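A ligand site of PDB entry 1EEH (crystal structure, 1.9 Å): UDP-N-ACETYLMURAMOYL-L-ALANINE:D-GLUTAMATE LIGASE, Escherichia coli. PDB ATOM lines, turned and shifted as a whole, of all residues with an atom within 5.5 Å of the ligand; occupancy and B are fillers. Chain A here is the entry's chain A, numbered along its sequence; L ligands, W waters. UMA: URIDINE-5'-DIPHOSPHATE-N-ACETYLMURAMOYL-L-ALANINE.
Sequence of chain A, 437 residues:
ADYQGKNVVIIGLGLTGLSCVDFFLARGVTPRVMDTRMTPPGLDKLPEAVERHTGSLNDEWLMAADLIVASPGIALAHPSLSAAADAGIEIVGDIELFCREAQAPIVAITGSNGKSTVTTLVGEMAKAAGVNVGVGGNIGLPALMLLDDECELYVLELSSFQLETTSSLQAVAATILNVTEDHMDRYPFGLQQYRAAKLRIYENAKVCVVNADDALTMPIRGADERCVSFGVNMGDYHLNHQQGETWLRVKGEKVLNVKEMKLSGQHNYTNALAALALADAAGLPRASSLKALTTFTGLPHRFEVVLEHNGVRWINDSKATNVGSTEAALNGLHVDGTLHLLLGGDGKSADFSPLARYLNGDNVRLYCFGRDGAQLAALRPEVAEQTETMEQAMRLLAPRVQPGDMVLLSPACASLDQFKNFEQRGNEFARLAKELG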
ATOM      1  N   ILE A  11      -5.932 -12.510  10.365  1.00  0.00           N
ATOM      2  CA  ILE A  11      -6.363 -11.113  10.521  1.00  0.00           C
ATOM      3  C   ILE A  11      -5.104 -10.314  10.786  1.00  0.00           C
ATOM      4  O   ILE A  11      -4.394 -10.572  11.749  1.00  0.00           O
ATOM      5  CB  ILE A  11      -7.304 -10.921  11.735  1.00  0.00           C
ATOM      6  CG1 ILE A  11      -8.566 -11.771  11.556  1.00  0.00           C
ATOM      7  CG2 ILE A  11      -7.666  -9.435  11.882  1.00  0.00           C
ATOM      8  CD1 ILE A  11      -9.509 -11.707  12.755  1.00  0.00           C
ATOM      9  N   GLY A  12      -4.830  -9.341   9.920  1.00  0.00           N
ATOM     10  CA  GLY A  12      -3.652  -8.507  10.093  1.00  0.00           C
ATOM     11  C   GLY A  12      -2.626  -8.814   9.033  1.00  0.00           C
ATOM     12  O   GLY A  12      -2.169  -9.951   8.923  1.00  0.00           O
ATOM     13  N   LEU A  13      -2.275  -7.792   8.247  1.00  0.00           N
ATOM     14  CA  LEU A  13      -1.309  -7.935   7.166  1.00  0.00           C
ATOM     15  C   LEU A  13      -0.050  -7.110   7.446  1.00  0.00           C
ATOM     16  O   LEU A  13       0.479  -6.448   6.547  1.00  0.00           O
ATOM     17  CB  LEU A  13      -1.910  -7.504   5.816  1.00  0.00           C
ATOM     18  CG  LEU A  13      -2.799  -8.526   5.092  1.00  0.00           C
ATOM     19  CD1 LEU A  13      -3.506  -7.913   3.879  1.00  0.00           C
ATOM     20  CD2 LEU A  13      -1.920  -9.712   4.666  1.00  0.00           C
ATOM     21  N   GLY A  14       0.409  -7.144   8.682  1.00  0.00           N
ATOM     22  CA  GLY A  14       1.627  -6.440   9.033  1.00  0.00           C
ATOM     23  C   GLY A  14       2.730  -7.475   9.036  1.00  0.00           C
ATOM     24  O   GLY A  14       2.615  -8.495   8.341  1.00  0.00           O
ATOM     25  N   LEU A  15       3.785  -7.239   9.813  1.00  0.00           N
ATOM     26  CA  LEU A  15       4.901  -8.177   9.880  1.00  0.00           C
ATOM     27  C   LEU A  15       4.449  -9.561  10.323  1.00  0.00           C
ATOM     28  O   LEU A  15       4.838 -10.558   9.730  1.00  0.00           O
ATOM     29  CB  LEU A  15       5.956  -7.676  10.866  1.00  0.00           C
ATOM     30  CG  LEU A  15       6.290  -6.190  10.769  1.00  0.00           C
ATOM     31  CD1 LEU A  15       7.518  -5.896  11.616  1.00  0.00           C
ATOM     32  CD2 LEU A  15       6.536  -5.802   9.323  1.00  0.00           C
ATOM     33  N   THR A  16       3.636  -9.603  11.373  1.00  0.00           N
ATOM     34  CA  THR A  16       3.131 -10.871  11.901  1.00  0.00           C
ATOM     35  C   THR A  16       2.262 -11.573  10.888  1.00  0.00           C
ATOM     36  O   THR A  16       2.408 -12.769  10.641  1.00  0.00           O
ATOM     37  CB  THR A  16       2.288 -10.653  13.166  1.00  0.00           C
ATOM     38  OG1 THR A  16       3.095 -10.034  14.178  1.00  0.00           O
ATOM     39  CG2 THR A  16       1.745 -11.991  13.679  1.00  0.00           C
ATOM     40  N   GLY A  17       1.333 -10.837  10.303  1.00  0.00           N
ATOM     41  CA  GLY A  17       0.426 -11.441   9.354  1.00  0.00           C
ATOM     42  C   GLY A  17       1.151 -12.073   8.194  1.00  0.00           C
ATOM     43  O   GLY A  17       0.819 -13.180   7.764  1.00  0.00           O
ATOM     44  N   MET A  34      -7.243 -10.819   5.990  1.00  0.00           N
ATOM     45  CA  MET A  34      -7.968  -9.557   6.053  1.00  0.00           C
ATOM     46  C   MET A  34      -7.287  -8.607   7.031  1.00  0.00           C
ATOM     47  O   MET A  34      -6.480  -9.016   7.852  1.00  0.00           O
ATOM     48  CB  MET A  34      -9.407  -9.795   6.524  1.00  0.00           C
ATOM     49  CG  MET A  34      -9.499 -10.409   7.903  1.00  0.00           C
ATOM     50  SD  MET A  34     -11.200 -10.725   8.401  1.00  0.00           S
ATOM     51  CE  MET A  34     -11.644 -12.118   7.350  1.00  0.00           C
ATOM     52  N   ASP A  35      -7.642  -7.335   6.925  1.00  0.00           N
ATOM     53  CA  ASP A  35      -7.084  -6.304   7.800  1.00  0.00           C
ATOM     54  C   ASP A  35      -8.057  -5.125   7.759  1.00  0.00           C
ATOM     55  O   ASP A  35      -8.562  -4.811   6.678  1.00  0.00           O
ATOM     56  CB  ASP A  35      -5.716  -5.873   7.289  1.00  0.00           C
ATOM     57  CG  ASP A  35      -4.926  -5.046   8.322  1.00  0.00           C
ATOM     58  OD1 ASP A  35      -5.413  -3.958   8.748  1.00  0.00           O
ATOM     59  OD2 ASP A  35      -3.820  -5.514   8.694  1.00  0.00           O
ATOM     60  N   THR A  36      -8.339  -4.484   8.887  1.00  0.00           N
ATOM     61  CA  THR A  36      -9.261  -3.343   8.861  1.00  0.00           C
ATOM     62  C   THR A  36      -8.645  -2.152   8.158  1.00  0.00           C
ATOM     63  O   THR A  36      -9.364  -1.255   7.710  1.00  0.00           O
ATOM     64  CB  THR A  36      -9.725  -2.897  10.274  1.00  0.00           C
ATOM     65  OG1 THR A  36      -8.610  -2.414  11.035  1.00  0.00           O
ATOM     66  CG2 THR A  36     -10.378  -4.073  11.008  1.00  0.00           C
ATOM     67  N   ARG A  37      -7.318  -2.113   8.094  1.00  0.00           N
ATOM     68  CA  ARG A  37      -6.631  -1.023   7.382  1.00  0.00           C
ATOM     69  C   ARG A  37      -6.813  -1.221   5.871  1.00  0.00           C
ATOM     70  O   ARG A  37      -6.715  -2.356   5.375  1.00  0.00           O
ATOM     71  CB  ARG A  37      -5.144  -1.029   7.715  1.00  0.00           C
ATOM     72  CG  ARG A  37      -4.807  -0.634   9.172  1.00  0.00           C
ATOM     73  CD  ARG A  37      -3.342  -0.909   9.504  1.00  0.00           C
ATOM     74  NE  ARG A  37      -3.070  -2.333   9.568  1.00  0.00           N
ATOM     75  CZ  ARG A  37      -1.879  -2.850   9.814  1.00  0.00           C
ATOM     76  NH1 ARG A  37      -0.838  -2.055  10.017  1.00  0.00           N
ATOM     77  NH2 ARG A  37      -1.719  -4.171   9.828  1.00  0.00           N
ATOM     78  N   LEU A  57     -13.261  -6.060   8.373  1.00  0.00           N
ATOM     79  CA  LEU A  57     -13.136  -7.499   8.514  1.00  0.00           C
ATOM     80  C   LEU A  57     -14.222  -8.104   7.666  1.00  0.00           C
ATOM     81  O   LEU A  57     -15.232  -7.450   7.399  1.00  0.00           O
ATOM     82  CB  LEU A  57     -13.321  -7.940   9.963  1.00  0.00           C
ATOM     83  CG  LEU A  57     -12.309  -7.421  10.989  1.00  0.00           C
ATOM     84  CD1 LEU A  57     -12.638  -7.995  12.380  1.00  0.00           C
ATOM     85  CD2 LEU A  57     -10.888  -7.809  10.562  1.00  0.00           C
ATOM     86  N   SER A  71      -3.607 -11.334  14.524  1.00  0.00           N
ATOM     87  CA  SER A  71      -2.398 -10.573  14.805  1.00  0.00           C
ATOM     88  C   SER A  71      -2.584  -9.900  16.168  1.00  0.00           C
ATOM     89  O   SER A  71      -3.707  -9.690  16.620  1.00  0.00           O
ATOM     90  CB  SER A  71      -2.166  -9.516  13.699  1.00  0.00           C
ATOM     91  OG  SER A  71      -1.841 -10.151  12.468  1.00  0.00           O
ATOM     92  N   PRO A  72      -1.484  -9.544  16.836  1.00  0.00           N
ATOM     93  CA  PRO A  72      -1.573  -8.902  18.154  1.00  0.00           C
ATOM     94  C   PRO A  72      -2.315  -7.576  18.125  1.00  0.00           C
ATOM     95  O   PRO A  72      -2.866  -7.167  19.127  1.00  0.00           O
ATOM     96  CB  PRO A  72      -0.113  -8.674  18.555  1.00  0.00           C
ATOM     97  CG  PRO A  72       0.666  -9.626  17.702  1.00  0.00           C
ATOM     98  CD  PRO A  72      -0.083  -9.689  16.400  1.00  0.00           C
ATOM     99  N   GLY A  73      -2.310  -6.929  16.971  1.00  0.00           N
ATOM    100  CA  GLY A  73      -2.937  -5.624  16.827  1.00  0.00           C
ATOM    101  C   GLY A  73      -4.456  -5.548  16.827  1.00  0.00           C
ATOM    102  O   GLY A  73      -5.008  -4.454  16.734  1.00  0.00           O
ATOM    103  N   ILE A  74      -5.125  -6.685  16.881  1.00  0.00           N
ATOM    104  CA  ILE A  74      -6.576  -6.678  16.908  1.00  0.00           C
ATOM    105  C   ILE A  74      -6.964  -7.379  18.213  1.00  0.00           C
ATOM    106  O   ILE A  74      -6.345  -8.369  18.594  1.00  0.00           O
ATOM    107  CB  ILE A  74      -7.198  -7.379  15.675  1.00  0.00           C
ATOM    108  CG1 ILE A  74      -8.699  -7.074  15.634  1.00  0.00           C
ATOM    109  CG2 ILE A  74      -6.984  -8.892  15.717  1.00  0.00           C
ATOM    110  CD1 ILE A  74      -9.333  -7.396  14.316  1.00  0.00           C
ATOM    111  N   ASP A  94       0.406 -15.737  16.228  1.00  0.00           N
ATOM    112  CA  ASP A  94       1.649 -16.288  15.689  1.00  0.00           C
ATOM    113  C   ASP A  94       2.512 -17.007  16.734  1.00  0.00           C
ATOM    114  O   ASP A  94       3.181 -17.978  16.415  1.00  0.00           O
ATOM    115  CB  ASP A  94       2.451 -15.175  14.990  1.00  0.00           C
ATOM    116  CG  ASP A  94       3.118 -14.222  15.969  1.00  0.00           C
ATOM    117  OD1 ASP A  94       2.442 -13.710  16.871  1.00  0.00           O
ATOM    118  OD2 ASP A  94       4.342 -13.953  15.824  1.00  0.00           O
ATOM    119  N   LYS A 115      11.948  -4.176  28.302  1.00  0.00           N
ATOM    120  CA  LYS A 115      11.765  -5.564  27.878  1.00  0.00           C
ATOM    121  C   LYS A 115      12.823  -5.978  26.873  1.00  0.00           C
ATOM    122  O   LYS A 115      13.441  -7.024  26.997  1.00  0.00           O
ATOM    123  CB  LYS A 115      10.395  -5.761  27.214  1.00  0.00           C
ATOM    124  CG  LYS A 115       9.204  -5.781  28.147  1.00  0.00           C
ATOM    125  CD  LYS A 115       8.033  -6.543  27.524  1.00  0.00           C
ATOM    126  CE  LYS A 115       7.515  -5.875  26.261  1.00  0.00           C
ATOM    127  NZ  LYS A 115       6.917  -4.537  26.552  1.00  0.00           N
ATOM    128  N   GLY A 137      10.323 -12.146  18.398  1.00  0.00           N
ATOM    129  CA  GLY A 137       9.057 -11.833  19.017  1.00  0.00           C
ATOM    130  C   GLY A 137       8.737 -10.358  18.867  1.00  0.00           C
ATOM    131  O   GLY A 137       9.042  -9.735  17.850  1.00  0.00           O
ATOM    132  N   ASN A 138       8.112  -9.802  19.898  1.00  0.00           N
ATOM    133  CA  ASN A 138       7.695  -8.398  19.889  1.00  0.00           C
ATOM    134  C   ASN A 138       8.895  -7.470  19.708  1.00  0.00           C
ATOM    135  O   ASN A 138       8.743  -6.309  19.326  1.00  0.00           O
ATOM    136  CB  ASN A 138       6.958  -8.083  21.198  1.00  0.00           C
ATOM    137  CG  ASN A 138       6.179  -6.780  21.135  1.00  0.00           C
ATOM    138  OD1 ASN A 138       5.341  -6.580  20.256  1.00  0.00           O
ATOM    139  ND2 ASN A 138       6.443  -5.877  22.062  1.00  0.00           N
ATOM    140  N   ILE A 139      10.084  -7.997  19.956  1.00  0.00           N
ATOM    141  CA  ILE A 139      11.302  -7.205  19.832  1.00  0.00           C
ATOM    142  C   ILE A 139      11.571  -6.780  18.389  1.00  0.00           C
ATOM    143  O   ILE A 139      12.313  -5.827  18.161  1.00  0.00           O
ATOM    144  CB  ILE A 139      12.518  -7.957  20.407  1.00  0.00           C
ATOM    145  CG1 ILE A 139      13.731  -7.019  20.484  1.00  0.00           C
ATOM    146  CG2 ILE A 139      12.823  -9.182  19.562  1.00  0.00           C
ATOM    147  CD1 ILE A 139      14.939  -7.613  21.215  1.00  0.00           C
ATOM    148  N   GLY A 140      10.989  -7.485  17.414  1.00  0.00           N
ATOM    149  CA  GLY A 140      11.212  -7.098  16.030  1.00  0.00           C
ATOM    150  C   GLY A 140      11.071  -8.166  14.962  1.00  0.00           C
ATOM    151  O   GLY A 140      10.365  -7.978  13.977  1.00  0.00           O
ATOM    152  N   LEU A 141      11.775  -9.268  15.136  1.00  0.00           N
ATOM    153  CA  LEU A 141      11.694 -10.343  14.170  1.00  0.00           C
ATOM    154  C   LEU A 141      10.595 -11.290  14.597  1.00  0.00           C
ATOM    155  O   LEU A 141      10.695 -11.910  15.648  1.00  0.00           O
ATOM    156  CB  LEU A 141      13.027 -11.101  14.119  1.00  0.00           C
ATOM    157  CG  LEU A 141      13.095 -12.244  13.124  1.00  0.00           C
ATOM    158  CD1 LEU A 141      12.835 -11.728  11.711  1.00  0.00           C
ATOM    159  CD2 LEU A 141      14.476 -12.882  13.207  1.00  0.00           C
ATOM    160  N   PRO A 142       9.526 -11.390  13.807  1.00  0.00           N
ATOM    161  CA  PRO A 142       8.410 -12.273  14.141  1.00  0.00           C
ATOM    162  C   PRO A 142       8.942 -13.668  14.475  1.00  0.00           C
ATOM    163  O   PRO A 142       9.763 -14.221  13.729  1.00  0.00           O
ATOM    164  CB  PRO A 142       7.572 -12.258  12.872  1.00  0.00           C
ATOM    165  CG  PRO A 142       7.770 -10.866  12.347  1.00  0.00           C
ATOM    166  CD  PRO A 142       9.276 -10.684  12.525  1.00  0.00           C
ATOM    167  N   ALA A 143       8.473 -14.223  15.590  1.00  0.00           N
ATOM    168  CA  ALA A 143       8.911 -15.537  16.044  1.00  0.00           C
ATOM    169  C   ALA A 143       8.956 -16.614  14.963  1.00  0.00           C
ATOM    170  O   ALA A 143       9.922 -17.371  14.880  1.00  0.00           O
ATOM    171  CB  ALA A 143       8.026 -16.027  17.221  1.00  0.00           C
ATOM    172  N   GLU A 157      10.627 -11.887  23.293  1.00  0.00           N
ATOM    173  CA  GLU A 157      10.068 -10.769  24.024  1.00  0.00           C
ATOM    174  C   GLU A 157       8.600 -10.895  23.601  1.00  0.00           C
ATOM    175  O   GLU A 157       8.309 -10.978  22.410  1.00  0.00           O
ATOM    176  CB  GLU A 157      10.620  -9.437  23.533  1.00  0.00           C
ATOM    177  CG  GLU A 157      10.037  -8.231  24.262  1.00  0.00           C
ATOM    178  CD  GLU A 157      10.256  -6.926  23.498  1.00  0.00           C
ATOM    179  OE1 GLU A 157      11.414  -6.678  23.097  1.00  0.00           O
ATOM    180  OE2 GLU A 157       9.288  -6.155  23.307  1.00  0.00           O
ATOM    181  N   SER A 159       4.455  -9.519  24.076  1.00  0.00           N
ATOM    182  CA  SER A 159       3.553  -8.485  24.548  1.00  0.00           C
ATOM    183  C   SER A 159       2.331  -9.164  25.182  1.00  0.00           C
ATOM    184  O   SER A 159       2.054 -10.345  24.959  1.00  0.00           O
ATOM    185  CB  SER A 159       3.073  -7.630  23.384  1.00  0.00           C
ATOM    186  OG  SER A 159       2.338  -8.413  22.443  1.00  0.00           O
ATOM    187  N   PHE A 161      -0.520  -8.623  24.303  1.00  0.00           N
ATOM    188  CA  PHE A 161      -1.373  -8.963  23.153  1.00  0.00           C
ATOM    189  C   PHE A 161      -1.063 -10.385  22.647  1.00  0.00           C
ATOM    190  O   PHE A 161      -1.969 -11.194  22.449  1.00  0.00           O
ATOM    191  CB  PHE A 161      -1.182  -7.973  22.003  1.00  0.00           C
ATOM    192  CG  PHE A 161      -1.443  -6.525  22.364  1.00  0.00           C
ATOM    193  CD1 PHE A 161      -2.358  -6.183  23.363  1.00  0.00           C
ATOM    194  CD2 PHE A 161      -0.791  -5.499  21.664  1.00  0.00           C
ATOM    195  CE1 PHE A 161      -2.638  -4.829  23.668  1.00  0.00           C
ATOM    196  CE2 PHE A 161      -1.050  -4.142  21.958  1.00  0.00           C
ATOM    197  CZ  PHE A 161      -1.980  -3.806  22.960  1.00  0.00           C
ATOM    198  N   GLN A 162       0.212 -10.678  22.440  1.00  0.00           N
ATOM    199  CA  GLN A 162       0.602 -12.007  21.944  1.00  0.00           C
ATOM    200  C   GLN A 162       0.262 -13.061  22.977  1.00  0.00           C
ATOM    201  O   GLN A 162      -0.166 -14.179  22.638  1.00  0.00           O
ATOM    202  CB  GLN A 162       2.104 -12.029  21.655  1.00  0.00           C
ATOM    203  CG  GLN A 162       2.527 -11.088  20.533  1.00  0.00           C
ATOM    204  CD  GLN A 162       4.029 -10.902  20.439  1.00  0.00           C
ATOM    205  OE1 GLN A 162       4.689 -10.717  21.448  1.00  0.00           O
ATOM    206  NE2 GLN A 162       4.557 -10.921  19.219  1.00  0.00           N
ATOM    207  N   HIS A 183      -1.451   0.757  26.903  1.00  0.00           N
ATOM    208  CA  HIS A 183      -2.371   0.163  25.940  1.00  0.00           C
ATOM    209  C   HIS A 183      -3.700  -0.167  26.627  1.00  0.00           C
ATOM    210  O   HIS A 183      -4.380  -1.135  26.270  1.00  0.00           O
ATOM    211  CB  HIS A 183      -1.763  -1.120  25.341  1.00  0.00           C
ATOM    212  CG  HIS A 183      -0.623  -0.870  24.407  1.00  0.00           C
ATOM    213  ND1 HIS A 183      -0.759  -0.136  23.241  1.00  0.00           N
ATOM    214  CD2 HIS A 183       0.675  -1.246  24.465  1.00  0.00           C
ATOM    215  CE1 HIS A 183       0.405  -0.083  22.620  1.00  0.00           C
ATOM    216  NE2 HIS A 183       1.300  -0.743  23.346  1.00  0.00           N
HETATM  217  N1  UMA L   1      -4.312  -3.183  12.906  1.00  0.00           N
HETATM  218  C2  UMA L   1      -5.554  -2.656  12.417  1.00  0.00           C
HETATM  219  N3  UMA L   1      -6.378  -3.605  11.820  1.00  0.00           N
HETATM  220  C4  UMA L   1      -6.091  -4.962  11.669  1.00  0.00           C
HETATM  221  C5  UMA L   1      -4.805  -5.438  12.184  1.00  0.00           C
HETATM  222  C6  UMA L   1      -3.959  -4.555  12.785  1.00  0.00           C
HETATM  223  O2  UMA L   1      -5.906  -1.461  12.504  1.00  0.00           O
HETATM  224  O4  UMA L   1      -6.918  -5.662  11.140  1.00  0.00           O
HETATM  225  C1B UMA L   1      -3.358  -2.191  13.400  1.00  0.00           C
HETATM  226  C2B UMA L   1      -3.005  -2.384  14.872  1.00  0.00           C
HETATM  227  O2' UMA L   1      -4.081  -1.726  15.669  1.00  0.00           O
HETATM  228  C3B UMA L   1      -1.711  -1.672  14.945  1.00  0.00           C
HETATM  229  C4B UMA L   1      -1.042  -1.943  13.593  1.00  0.00           C
HETATM  230  O4B UMA L   1      -2.161  -2.109  12.672  1.00  0.00           O
HETATM  231  O3B UMA L   1      -1.962  -0.270  14.934  1.00  0.00           O
HETATM  232  C5B UMA L   1      -0.046  -3.127  13.588  1.00  0.00           C
HETATM  233  O5B UMA L   1      -0.673  -4.383  14.029  1.00  0.00           O
HETATM  234  PA  UMA L   1      -0.107  -5.765  13.585  1.00  0.00           P
HETATM  235  O1A UMA L   1      -0.717  -6.827  14.426  1.00  0.00           O
HETATM  236  O2A UMA L   1      -0.130  -5.958  12.129  1.00  0.00           O
HETATM  237  O3A UMA L   1       1.447  -5.613  14.011  1.00  0.00           O
HETATM  238  PB  UMA L   1       2.792  -6.127  13.324  1.00  0.00           P
HETATM  239  O1B UMA L   1       3.227  -5.224  12.266  1.00  0.00           O
HETATM  240  O2B UMA L   1       2.701  -7.623  13.041  1.00  0.00           O
HETATM  241  O1' UMA L   1       3.801  -5.976  14.551  1.00  0.00           O
HETATM  242  C1' UMA L   1       3.561  -6.770  15.730  1.00  0.00           C
HETATM  243  C2' UMA L   1       3.872  -5.894  16.956  1.00  0.00           C
HETATM  244  N2' UMA L   1       2.964  -4.766  17.012  1.00  0.00           N
HETATM  245  C7' UMA L   1       1.826  -4.841  17.729  1.00  0.00           C
HETATM  246  O7' UMA L   1       1.552  -5.805  18.512  1.00  0.00           O
HETATM  247  C8' UMA L   1       0.821  -3.713  17.550  1.00  0.00           C
HETATM  248  C3' UMA L   1       5.360  -5.468  16.846  1.00  0.00           C
HETATM  249  O3' UMA L   1       5.702  -4.654  17.935  1.00  0.00           O
HETATM  250  C4' UMA L   1       6.247  -6.716  16.835  1.00  0.00           C
HETATM  251  O4' UMA L   1       7.612  -6.364  16.753  1.00  0.00           O
HETATM  252  C5' UMA L   1       5.873  -7.587  15.625  1.00  0.00           C
HETATM  253  O5' UMA L   1       4.441  -7.933  15.679  1.00  0.00           O
HETATM  254  C6' UMA L   1       6.656  -8.903  15.602  1.00  0.00           C
HETATM  255  O6' UMA L   1       6.255  -9.711  16.727  1.00  0.00           O
HETATM  256  C18 UMA L   1       5.755  -3.208  17.955  1.00  0.00           C
HETATM  257  C19 UMA L   1       4.778  -2.661  18.968  1.00  0.00           C
HETATM  258  O18 UMA L   1       4.461  -1.471  18.979  1.00  0.00           O
HETATM  259  C20 UMA L   1       7.194  -2.746  18.071  1.00  0.00           C
HETATM  260  N4  UMA L   1       4.303  -3.560  19.847  1.00  0.00           N
HETATM  261  C21 UMA L   1       3.673  -3.204  21.115  1.00  0.00           C
HETATM  262  C22 UMA L   1       4.712  -2.751  22.188  1.00  0.00           C
HETATM  263  O19 UMA L   1       5.869  -3.286  22.216  1.00  0.00           O
HETATM  264  O20 UMA L   1       4.388  -1.843  22.976  1.00  0.00           O
HETATM  265  C23 UMA L   1       2.805  -4.339  21.638  1.00  0.00           C
HETATM  266  O   HOH W   1      -7.073  -3.146  15.391  1.00  0.00           O
HETATM  267  O   HOH W   2      -0.219  -8.333  11.131  1.00  0.00           O
HETATM  268  O   HOH W   3       8.643  -4.726  14.924  1.00  0.00           O
HETATM  269  O   HOH W   4      -6.565   1.105  13.389  1.00  0.00           O
HETATM  270  O   HOH W   5      -2.401  -2.146  18.531  1.00  0.00           O
HETATM  271  O   HOH W   6       2.032  -3.180  10.565  1.00  0.00           O
HETATM  272  O   HOH W   7       6.445 -12.527  16.792  1.00  0.00           O
HETATM  273  O   HOH W   8       3.342 -11.021  16.772  1.00  0.00           O
HETATM  274  O   HOH W   9       2.789  -7.655  19.979  1.00  0.00           O
HETATM  275  O   HOH W  10       3.481  -2.316  15.090  1.00  0.00           O
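N of Thr 36 lies within hydrogen-bond range of O4 of the ligand.
A nitrogen (N3) of the ligand sits at hydrogen-bond distance from the side-chain hydroxyl of Thr 36 (2.6 Å).
The backbone carbonyl oxygen (O) of Asn 138 lies within hydrogen-bond range of an oxygen (O4') of the ligand, 2.8 Å away.
The side-chain amide nitrogen of Asn 138 is in hydrogen-bond range of an oxygen (O19) of the ligand, at 2.7 Å.
The backbone NH (N) of Thr 16 is in hydrogen-bond range of an oxygen (O2B) of the ligand (2.8 Å).
An oxygen (O2B) of the ligand lies within hydrogen-bond range of the side-chain hydroxyl (OG1) of Thr 16 (2.7 Å).
NH2 of Arg 37 is in salt-bridge range of O2A of the ligand (3.3 Å).
O of Gly 137 is in hydrogen-bond range of O6' of the ligand (3.0 Å).
The backbone NH (N) of Gly 73 sits at hydrogen-bond distance from an oxygen (O1A) of the ligand, at 3.0 Å.
The backbone carbonyl oxygen (O) of Gly 73 lies within hydrogen-bond range of an oxygen (O2') of the ligand (3.1 Å).
The side-chain carboxylate (OD1) of Asp 35 lies close to a nitrogen (N3) of the ligand, 3.2 Å away.
The backbone NH of Leu 15 sits at hydrogen-bond distance from an oxygen (O1B) of the ligand (3.2 Å).
O6' of the ligand lies within hydrogen-bond range of NE2 of Gln 162, 3.2 Å away.
An oxygen (O20) of the ligand lies within hydrogen-bond range of a ring nitrogen (NE2) of His 183, 3.3 Å away.
The backbone carbonyl oxygen of Glu 157 lies within hydrogen-bond range of the backbone NH of Asn 138, at 2.8 Å.
The guanidinium group (NH2) of Arg 37 lies within salt-bridge range of the side-chain carboxylate (OD2) of Asp 35, at 2.7 Å.
OG of Ser 71 is in hydrogen-bond range of O of Ile 11 (2.7 Å).
The backbone NH (N) of Leu 13 is in hydrogen-bond range of the side-chain carboxylate (OD2) of Asp 35 (2.8 Å).
N of Ser 159 is in hydrogen-bond range of OE1 of Gln 162 (2.9 Å).
OG of Ser 159 sits close to N of Phe 161 (3.4 Å).
The backbone NH (N) of Gly 12 lies within hydrogen-bond range of the backbone carbonyl oxygen (O) of Met 34 (2.7 Å).
Ile 11 touches the ligand (CG2 to O4, 3.9 Å).
CA of Gly 12 touches C5 of the ligand, 3.9 Å away.
CA of Gly 14 touches O2A of the ligand, at 3.6 Å.
Ser 71 touches the ligand.
Pro 72 touches the ligand (CB to O7', 3.3 Å).
Gly 140 touches the ligand.
Pro 142 touches the ligand (CG to C6', 3.96 Å).
CB of Ser 159 touches C23 of the ligand (3.7 Å).
Phe 161 touches the ligand (CD2 to C23, 3.8 Å).
Within 4 Å of the ligand: Ile 11, Gly 12, Gly 14, Leu 15, Thr 16, Asp 35, Thr 36, Arg 37, Ser 71, Pro 72, Gly 73, Gly 137, Asn 138, Gly 140, Pro 142, Ser 159, Phe 161, Gln 162 and His 183.
Water W2 lies within hydrogen-bond range of an oxygen (O2A) of the ligand, the side-chain hydroxyl of Ser 71, the backbone NH of Gly 14, the backbone NH of Gly 17 and the backbone carbonyl oxygen of Gly 12.
Water W9 lies within hydrogen-bond range of the side-chain hydroxyl of Ser 159 (2.6 Å), an oxygen (O7') of the ligand (2.7 Å) and the side-chain amide oxygen of Asn 138 (2.8 Å).
Water W7 lies within hydrogen-bond range of the side-chain carboxylate (OD2) of Asp 94 (2.7 Å), an oxygen (O6') of the ligand (2.8 Å), the backbone NH (N) of Ala 143 (2.9 Å) and the side-chain amide nitrogen (NE2) of Gln 162 (3.5 Å).
Water W6 lies within hydrogen-bond range of an oxygen (O1B) of the ligand and the guanidinium group (NH1) of Arg 37.
Water W8 lies within hydrogen-bond range of NE2 of Gln 162 (2.7 Å), OG1 of Thr 16 (2.8 Å), OD1 of Asp 94 (2.8 Å) and O6' of the ligand (3.2 Å).
Water W1 bridges O of Gly 73 (2.8 Å) and O2' of the ligand (3.3 Å).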
